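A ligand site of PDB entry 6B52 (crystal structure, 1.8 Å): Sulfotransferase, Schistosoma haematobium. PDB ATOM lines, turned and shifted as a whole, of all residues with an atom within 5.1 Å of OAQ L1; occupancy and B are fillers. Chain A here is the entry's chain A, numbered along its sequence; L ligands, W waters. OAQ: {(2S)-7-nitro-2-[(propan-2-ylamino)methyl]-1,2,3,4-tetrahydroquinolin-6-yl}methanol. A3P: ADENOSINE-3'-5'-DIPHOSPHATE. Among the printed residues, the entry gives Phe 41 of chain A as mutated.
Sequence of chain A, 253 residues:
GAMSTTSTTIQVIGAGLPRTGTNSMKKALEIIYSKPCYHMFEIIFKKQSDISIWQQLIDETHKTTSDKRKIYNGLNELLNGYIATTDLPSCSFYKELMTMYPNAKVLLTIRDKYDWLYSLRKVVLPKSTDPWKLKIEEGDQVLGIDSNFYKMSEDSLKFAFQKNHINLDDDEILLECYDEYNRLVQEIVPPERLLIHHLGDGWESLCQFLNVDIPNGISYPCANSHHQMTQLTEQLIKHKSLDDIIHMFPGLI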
ATOM      1  N   PRO A  18     -10.403   7.415  26.058  1.00  0.00           N
ATOM      2  CA  PRO A  18     -11.542   7.041  25.207  1.00  0.00           C
ATOM      3  C   PRO A  18     -11.097   6.233  23.973  1.00  0.00           C
ATOM      4  O   PRO A  18      -9.981   6.409  23.457  1.00  0.00           O
ATOM      5  CB  PRO A  18     -12.147   8.393  24.803  1.00  0.00           C
ATOM      6  CG  PRO A  18     -11.123   9.418  25.142  1.00  0.00           C
ATOM      7  CD  PRO A  18     -10.360   8.862  26.310  1.00  0.00           C
ATOM      8  N   THR A  22     -13.348   1.413  27.086  1.00  0.00           N
ATOM      9  CA  THR A  22     -13.742   1.905  28.409  1.00  0.00           C
ATOM     10  C   THR A  22     -15.202   1.543  28.715  1.00  0.00           C
ATOM     11  O   THR A  22     -15.517   1.238  29.862  1.00  0.00           O
ATOM     12  CB  THR A  22     -13.579   3.421  28.552  1.00  0.00           C
ATOM     13  OG1 THR A  22     -14.380   4.084  27.577  1.00  0.00           O
ATOM     14  CG2 THR A  22     -12.088   3.821  28.380  1.00  0.00           C
ATOM     15  N   HIS A  39     -18.732   6.769  33.366  1.00  0.00           N
ATOM     16  CA  HIS A  39     -18.282   6.719  31.976  1.00  0.00           C
ATOM     17  C   HIS A  39     -18.840   7.953  31.307  1.00  0.00           C
ATOM     18  O   HIS A  39     -19.794   8.534  31.831  1.00  0.00           O
ATOM     19  CB  HIS A  39     -18.757   5.440  31.289  1.00  0.00           C
ATOM     20  CG  HIS A  39     -18.179   5.222  29.926  1.00  0.00           C
ATOM     21  ND1 HIS A  39     -18.795   5.668  28.770  1.00  0.00           N
ATOM     22  CD2 HIS A  39     -17.055   4.568  29.528  1.00  0.00           C
ATOM     23  CE1 HIS A  39     -18.070   5.322  27.724  1.00  0.00           C
ATOM     24  NE2 HIS A  39     -17.012   4.646  28.146  1.00  0.00           N
ATOM     25  N   MET A  40     -18.271   8.371  30.172  1.00  0.00           N
ATOM     26  CA  MET A  40     -18.825   9.523  29.454  1.00  0.00           C
ATOM     27  C   MET A  40     -20.310   9.314  29.138  1.00  0.00           C
ATOM     28  O   MET A  40     -21.093  10.261  29.129  1.00  0.00           O
ATOM     29  CB  MET A  40     -18.045   9.807  28.168  1.00  0.00           C
ATOM     30  CG  MET A  40     -18.429  11.131  27.489  1.00  0.00           C
ATOM     31  SD  MET A  40     -18.079  12.568  28.519  1.00  0.00           S
ATOM     32  CE  MET A  40     -16.380  12.916  28.059  1.00  0.00           C
ATOM     33  N   PHE A  41     -20.697   8.065  28.895  1.00  0.00           N
ATOM     34  CA  PHE A  41     -22.094   7.752  28.581  1.00  0.00           C
ATOM     35  C   PHE A  41     -23.033   8.091  29.733  1.00  0.00           C
ATOM     36  O   PHE A  41     -24.216   8.372  29.504  1.00  0.00           O
ATOM     37  CB  PHE A  41     -22.233   6.271  28.200  1.00  0.00           C
ATOM     38  CG  PHE A  41     -21.891   5.961  26.771  1.00  0.00           C
ATOM     39  CD1 PHE A  41     -20.823   6.593  26.135  1.00  0.00           C
ATOM     40  CD2 PHE A  41     -22.602   4.987  26.069  1.00  0.00           C
ATOM     41  CE1 PHE A  41     -20.500   6.294  24.824  1.00  0.00           C
ATOM     42  CE2 PHE A  41     -22.276   4.681  24.753  1.00  0.00           C
ATOM     43  CZ  PHE A  41     -21.232   5.334  24.128  1.00  0.00           C
ATOM     44  N   ILE A  44     -23.579  11.834  29.021  1.00  0.00           N
ATOM     45  CA  ILE A  44     -24.320  12.116  27.789  1.00  0.00           C
ATOM     46  C   ILE A  44     -25.764  11.655  27.894  1.00  0.00           C
ATOM     47  O   ILE A  44     -26.688  12.367  27.491  1.00  0.00           O
ATOM     48  CB  ILE A  44     -23.670  11.421  26.572  1.00  0.00           C
ATOM     49  CG1 ILE A  44     -22.322  12.074  26.244  1.00  0.00           C
ATOM     50  CG2 ILE A  44     -24.575  11.511  25.353  1.00  0.00           C
ATOM     51  CD1 ILE A  44     -21.586  11.365  25.142  1.00  0.00           C
ATOM     52  N   PHE A  45     -25.969  10.480  28.467  1.00  0.00           N
ATOM     53  CA  PHE A  45     -27.293   9.880  28.365  1.00  0.00           C
ATOM     54  C   PHE A  45     -28.133   9.942  29.642  1.00  0.00           C
ATOM     55  O   PHE A  45     -29.338   9.737  29.601  1.00  0.00           O
ATOM     56  CB  PHE A  45     -27.150   8.431  27.907  1.00  0.00           C
ATOM     57  CG  PHE A  45     -26.658   8.285  26.477  1.00  0.00           C
ATOM     58  CD1 PHE A  45     -27.508   8.567  25.414  1.00  0.00           C
ATOM     59  CD2 PHE A  45     -25.379   7.850  26.209  1.00  0.00           C
ATOM     60  CE1 PHE A  45     -27.061   8.433  24.104  1.00  0.00           C
ATOM     61  CE2 PHE A  45     -24.929   7.704  24.918  1.00  0.00           C
ATOM     62  CZ  PHE A  45     -25.779   8.006  23.863  1.00  0.00           C
ATOM     63  N   ASP A  87     -13.121   6.182  31.368  1.00  0.00           N
ATOM     64  CA  ASP A  87     -13.301   7.140  30.286  1.00  0.00           C
ATOM     65  C   ASP A  87     -13.043   8.575  30.736  1.00  0.00           C
ATOM     66  O   ASP A  87     -12.950   8.863  31.933  1.00  0.00           O
ATOM     67  CB  ASP A  87     -14.735   7.032  29.730  1.00  0.00           C
ATOM     68  CG  ASP A  87     -14.876   7.525  28.308  1.00  0.00           C
ATOM     69  OD1 ASP A  87     -13.876   7.999  27.701  1.00  0.00           O
ATOM     70  OD2 ASP A  87     -16.005   7.424  27.801  1.00  0.00           O
ATOM     71  N   LEU A  88     -12.903   9.470  29.753  1.00  0.00           N
ATOM     72  CA  LEU A  88     -13.000  10.912  29.991  1.00  0.00           C
ATOM     73  C   LEU A  88     -14.384  11.227  30.563  1.00  0.00           C
ATOM     74  O   LEU A  88     -15.346  10.549  30.240  1.00  0.00           O
ATOM     75  CB  LEU A  88     -12.787  11.698  28.692  1.00  0.00           C
ATOM     76  CG  LEU A  88     -11.366  11.747  28.133  1.00  0.00           C
ATOM     77  CD1 LEU A  88     -11.352  12.570  26.850  1.00  0.00           C
ATOM     78  CD2 LEU A  88     -10.438  12.335  29.154  1.00  0.00           C
ATOM     79  N   VAL A 123     -15.310   8.942  15.993  1.00  0.00           N
ATOM     80  CA  VAL A 123     -16.344   9.002  17.029  1.00  0.00           C
ATOM     81  C   VAL A 123     -16.242  10.216  17.948  1.00  0.00           C
ATOM     82  O   VAL A 123     -17.257  10.870  18.215  1.00  0.00           O
ATOM     83  CB  VAL A 123     -16.300   7.735  17.919  1.00  0.00           C
ATOM     84  CG1 VAL A 123     -17.353   7.813  19.011  1.00  0.00           C
ATOM     85  CG2 VAL A 123     -16.497   6.492  17.072  1.00  0.00           C
ATOM     86  N   VAL A 124     -15.042  10.517  18.406  1.00  0.00           N
ATOM     87  CA  VAL A 124     -14.870  11.455  19.518  1.00  0.00           C
ATOM     88  C   VAL A 124     -14.277  12.800  19.097  1.00  0.00           C
ATOM     89  O   VAL A 124     -14.769  13.861  19.514  1.00  0.00           O
ATOM     90  CB  VAL A 124     -13.974  10.842  20.617  1.00  0.00           C
ATOM     91  CG1 VAL A 124     -13.582  11.879  21.645  1.00  0.00           C
ATOM     92  CG2 VAL A 124     -14.683   9.645  21.271  1.00  0.00           C
ATOM     93  N   ILE A 136     -21.894  14.541  13.305  1.00  0.00           N
ATOM     94  CA  ILE A 136     -21.855  14.245  14.734  1.00  0.00           C
ATOM     95  C   ILE A 136     -22.581  15.310  15.525  1.00  0.00           C
ATOM     96  O   ILE A 136     -23.420  14.997  16.385  1.00  0.00           O
ATOM     97  CB  ILE A 136     -20.406  14.131  15.240  1.00  0.00           C
ATOM     98  CG1 ILE A 136     -19.753  12.855  14.696  1.00  0.00           C
ATOM     99  CG2 ILE A 136     -20.365  14.142  16.756  1.00  0.00           C
ATOM    100  CD1 ILE A 136     -18.267  12.799  14.941  1.00  0.00           C
ATOM    101  N   ASP A 140     -25.966  14.973  17.747  1.00  0.00           N
ATOM    102  CA  ASP A 140     -25.849  15.297  19.169  1.00  0.00           C
ATOM    103  C   ASP A 140     -26.903  16.305  19.617  1.00  0.00           C
ATOM    104  O   ASP A 140     -27.350  16.270  20.757  1.00  0.00           O
ATOM    105  CB  ASP A 140     -24.447  15.836  19.484  1.00  0.00           C
ATOM    106  CG  ASP A 140     -23.382  14.749  19.508  1.00  0.00           C
ATOM    107  OD1 ASP A 140     -23.750  13.557  19.514  1.00  0.00           O
ATOM    108  OD2 ASP A 140     -22.189  15.106  19.531  1.00  0.00           O
ATOM    109  N   LEU A 143     -29.792  14.884  21.122  1.00  0.00           N
ATOM    110  CA  LEU A 143     -29.636  14.440  22.504  1.00  0.00           C
ATOM    111  C   LEU A 143     -29.511  15.607  23.466  1.00  0.00           C
ATOM    112  O   LEU A 143     -29.415  15.414  24.675  1.00  0.00           O
ATOM    113  CB  LEU A 143     -28.417  13.530  22.642  1.00  0.00           C
ATOM    114  CG  LEU A 143     -28.323  12.345  21.686  1.00  0.00           C
ATOM    115  CD1 LEU A 143     -26.967  11.676  21.836  1.00  0.00           C
ATOM    116  CD2 LEU A 143     -29.461  11.362  21.935  1.00  0.00           C
ATOM    117  N   PHE A 149     -20.764  20.739  26.000  1.00  0.00           N
ATOM    118  CA  PHE A 149     -20.229  19.397  26.102  1.00  0.00           C
ATOM    119  C   PHE A 149     -18.888  19.270  25.422  1.00  0.00           C
ATOM    120  O   PHE A 149     -17.940  18.743  25.986  1.00  0.00           O
ATOM    121  CB  PHE A 149     -21.176  18.367  25.488  1.00  0.00           C
ATOM    122  CG  PHE A 149     -20.600  16.978  25.459  1.00  0.00           C
ATOM    123  CD1 PHE A 149     -20.534  16.216  26.617  1.00  0.00           C
ATOM    124  CD2 PHE A 149     -20.058  16.458  24.294  1.00  0.00           C
ATOM    125  CE1 PHE A 149     -19.982  14.943  26.612  1.00  0.00           C
ATOM    126  CE2 PHE A 149     -19.509  15.198  24.271  1.00  0.00           C
ATOM    127  CZ  PHE A 149     -19.467  14.435  25.431  1.00  0.00           C
ATOM    128  N   SER A 153     -15.298  18.152  27.098  1.00  0.00           N
ATOM    129  CA  SER A 153     -14.602  16.934  26.688  1.00  0.00           C
ATOM    130  C   SER A 153     -13.222  17.216  26.088  1.00  0.00           C
ATOM    131  O   SER A 153     -12.267  16.486  26.352  1.00  0.00           O
ATOM    132  CB  SER A 153     -15.438  16.138  25.688  1.00  0.00           C
ATOM    133  OG  SER A 153     -16.042  16.983  24.738  1.00  0.00           O
ATOM    134  N   MET A 229     -21.478   3.436  16.523  1.00  0.00           N
ATOM    135  CA  MET A 229     -21.616   4.845  16.836  1.00  0.00           C
ATOM    136  C   MET A 229     -21.924   5.667  15.579  1.00  0.00           C
ATOM    137  O   MET A 229     -22.660   6.648  15.629  1.00  0.00           O
ATOM    138  CB  MET A 229     -20.357   5.372  17.536  1.00  0.00           C
ATOM    139  CG  MET A 229     -20.160   4.789  18.936  1.00  0.00           C
ATOM    140  SD  MET A 229     -21.612   5.022  19.967  1.00  0.00           S
ATOM    141  CE  MET A 229     -21.726   6.811  19.983  1.00  0.00           C
ATOM    142  N   LEU A 232     -25.565   5.121  15.028  1.00  0.00           N
ATOM    143  CA  LEU A 232     -26.343   5.931  15.959  1.00  0.00           C
ATOM    144  C   LEU A 232     -26.484   7.369  15.487  1.00  0.00           C
ATOM    145  O   LEU A 232     -27.579   7.927  15.502  1.00  0.00           O
ATOM    146  CB  LEU A 232     -25.716   5.897  17.377  1.00  0.00           C
ATOM    147  CG  LEU A 232     -26.486   6.691  18.447  1.00  0.00           C
ATOM    148  CD1 LEU A 232     -27.922   6.198  18.584  1.00  0.00           C
ATOM    149  CD2 LEU A 232     -25.775   6.640  19.778  1.00  0.00           C
ATOM    150  N   THR A 233     -25.381   7.977  15.057  1.00  0.00           N
ATOM    151  CA  THR A 233     -25.416   9.331  14.533  1.00  0.00           C
ATOM    152  C   THR A 233     -26.364   9.400  13.332  1.00  0.00           C
ATOM    153  O   THR A 233     -27.240  10.265  13.285  1.00  0.00           O
ATOM    154  CB  THR A 233     -24.001   9.835  14.126  1.00  0.00           C
ATOM    155  OG1 THR A 233     -23.214  10.002  15.312  1.00  0.00           O
ATOM    156  CG2 THR A 233     -24.072  11.171  13.418  1.00  0.00           C
ATOM    157  N   LEU A 236     -29.958   9.189  14.438  1.00  0.00           N
ATOM    158  CA  LEU A 236     -30.390  10.342  15.230  1.00  0.00           C
ATOM    159  C   LEU A 236     -30.763  11.474  14.290  1.00  0.00           C
ATOM    160  O   LEU A 236     -31.769  12.176  14.496  1.00  0.00           O
ATOM    161  CB  LEU A 236     -29.278  10.807  16.196  1.00  0.00           C
ATOM    162  CG  LEU A 236     -29.133  10.004  17.501  1.00  0.00           C
ATOM    163  CD1 LEU A 236     -27.913  10.464  18.286  1.00  0.00           C
ATOM    164  CD2 LEU A 236     -30.389  10.112  18.358  1.00  0.00           C
HETATM  165  C1  OAQ L   1     -17.656   9.705  23.860  1.00  0.00           C
HETATM  166  C2  OAQ L   1     -16.572  10.345  24.467  1.00  0.00           C
HETATM  167  C3  OAQ L   1     -16.315  11.685  24.104  1.00  0.00           C
HETATM  168  C4  OAQ L   1     -17.118  12.323  23.182  1.00  0.00           C
HETATM  169  C5  OAQ L   1     -18.187  11.690  22.594  1.00  0.00           C
HETATM  170  C6  OAQ L   1     -18.463  10.367  22.938  1.00  0.00           C
HETATM  171  C7  OAQ L   1     -19.870  11.603  20.766  1.00  0.00           C
HETATM  172  C8  OAQ L   1     -19.545  10.113  20.877  1.00  0.00           C
HETATM  173  C9  OAQ L   1     -19.516   9.707  22.342  1.00  0.00           C
HETATM  174  C10 OAQ L   1     -15.826   9.605  25.383  1.00  0.00           C
HETATM  175  C11 OAQ L   1     -21.356  11.846  21.073  1.00  0.00           C
HETATM  176  C12 OAQ L   1     -23.633   9.821  18.849  1.00  0.00           C
HETATM  177  C13 OAQ L   1     -23.741  10.351  21.295  1.00  0.00           C
HETATM  178  C14 OAQ L   1     -22.832  10.260  20.088  1.00  0.00           C
HETATM  179  N1  OAQ L   1     -18.956  12.376  21.646  1.00  0.00           N
HETATM  180  N2  OAQ L   1     -15.294  12.414  24.599  1.00  0.00           N
HETATM  181  N3  OAQ L   1     -22.159  11.552  19.870  1.00  0.00           N
HETATM  182  O1  OAQ L   1     -15.016  13.686  23.920  1.00  0.00           O
HETATM  183  O2  OAQ L   1     -14.445  12.016  25.715  1.00  0.00           O
HETATM  184  O3  OAQ L   1     -16.242   8.225  25.379  1.00  0.00           O
HETATM  185  P1  A3P L   2     -13.478   0.491  17.422  1.00  0.00           P
HETATM  186  O1P A3P L   2     -14.472  -0.515  16.872  1.00  0.00           O
HETATM  187  O2P A3P L   2     -12.176   0.395  16.653  1.00  0.00           O
HETATM  188  O3P A3P L   2     -14.038   1.891  17.333  1.00  0.00           O
HETATM  189  P2  A3P L   2     -14.525   2.973  24.165  1.00  0.00           P
HETATM  190  O4P A3P L   2     -15.696   2.264  24.859  1.00  0.00           O
HETATM  191  O5P A3P L   2     -13.518   3.485  25.142  1.00  0.00           O
HETATM  192  O6P A3P L   2     -15.106   4.096  23.340  1.00  0.00           O
HETATM  193  O5' A3P L   2     -13.845   1.875  23.240  1.00  0.00           O
HETATM  194  C5' A3P L   2     -14.484   1.566  22.002  1.00  0.00           C
HETATM  195  C4' A3P L   2     -13.568   0.676  21.202  1.00  0.00           C
HETATM  196  O4' A3P L   2     -13.243  -0.547  21.922  1.00  0.00           O
HETATM  197  C3' A3P L   2     -14.212   0.237  19.939  1.00  0.00           C
HETATM  198  O3' A3P L   2     -13.185   0.117  18.946  1.00  0.00           O
HETATM  199  C2' A3P L   2     -14.713  -1.107  20.291  1.00  0.00           C
HETATM  200  O2' A3P L   2     -15.019  -1.891  19.150  1.00  0.00           O
HETATM  201  C1' A3P L   2     -13.585  -1.655  21.083  1.00  0.00           C
HETATM  202  N9  A3P L   2     -13.941  -2.734  21.939  1.00  0.00           N
HETATM  203  C8  A3P L   2     -14.747  -2.661  23.000  1.00  0.00           C
HETATM  204  N7  A3P L   2     -14.838  -3.860  23.591  1.00  0.00           N
HETATM  205  C5  A3P L   2     -14.075  -4.753  22.897  1.00  0.00           C
HETATM  206  C6  A3P L   2     -13.773  -6.143  23.039  1.00  0.00           C
HETATM  207  N6  A3P L   2     -14.336  -6.921  24.073  1.00  0.00           N
HETATM  208  N1  A3P L   2     -12.935  -6.706  22.133  1.00  0.00           N
HETATM  209  C2  A3P L   2     -12.417  -5.990  21.138  1.00  0.00           C
HETATM  210  N3  A3P L   2     -12.669  -4.691  20.991  1.00  0.00           N
HETATM  211  C4  A3P L   2     -13.486  -4.024  21.839  1.00  0.00           C
HETATM  212  O   HOH W   1     -19.902  10.502  17.749  1.00  0.00           O
HETATM  213  O   HOH W   2     -24.123  12.242  16.811  1.00  0.00           O
HETATM  214  O   HOH W   3     -17.514  14.430  20.294  1.00  0.00           O
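Water W3 lies within hydrogen-bond range of N1 of OAQ L1 and O of Val 124. Water W1 lies within hydrogen-bond range of O of Val 123 and N3 of OAQ L1. Water W2 lies within hydrogen-bond range of the side-chain hydroxyl of Thr 233 (2.8 Å), the backbone carbonyl oxygen of Ile 136 (2.9 Å) and the side-chain carboxylate of Asp 140 (3.0 Å).
The backbone NH of Thr 22 lies within hydrogen-bond range of an oxygen (O5P) of A3P L2. A nitrogen (N3) of OAQ L1 lies within salt-bridge range of the side-chain carboxylate (OD1) of Asp 140. O3 of OAQ L1 sits at hydrogen-bond distance from OD2 of Asp 87. O5P of A3P L2 lies within hydrogen-bond range of OG1 of Thr 22 (2.7 Å).
The side-chain carboxylate (OD2) of Asp 87 lies close to the backbone NH (N) of Met 40 (3.4 Å). The side-chain hydroxyl (OG) of Ser 153 is in hydrogen-bond range of the backbone carbonyl oxygen (O) of Phe 149, 2.9 Å away. The side-chain carboxylate (OD2) of Asp 87 lies close to a ring nitrogen (NE2) of His 39 (3.0 Å). The side-chain hydroxyl of Thr 233 sits at hydrogen-bond distance from the backbone carbonyl oxygen of Met 229, 3.4 Å away.
CB of Pro 18 touches C10 of OAQ L1 (3.9 Å). CE of Met 40 touches O2 of OAQ L1, at 3.2 Å. CD1 of Ile 44 touches C9 of OAQ L1 (3.9 Å). Leu 88 touches OAQ L1. O of Val 123 touches C8 of OAQ L1, at 3.6 Å. Val 124 touches OAQ L1. Leu 143 touches OAQ L1. CZ of Phe 149 touches C4 of OAQ L1, at 3.9 Å. Ser 153 touches OAQ L1. Met 229 touches OAQ L1. Leu 232 touches OAQ L1. Thr 233 touches OAQ L1. Hydrophobic or aromatic side chains that line OAQ L1: Pro 18, Met 40, Ile 44, Leu 88, Val 123, Val 124, Leu 143, Phe 149, Met 229 and Leu 232. 14 residues have an atom within 4 Å of OAQ L1: Pro 18, Met 40, Ile 44, Asp 87, Leu 88, Val 123, Val 124, Asp 140, Leu 143, Phe 149, Ser 153, Met 229, Leu 232 and Thr 233.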
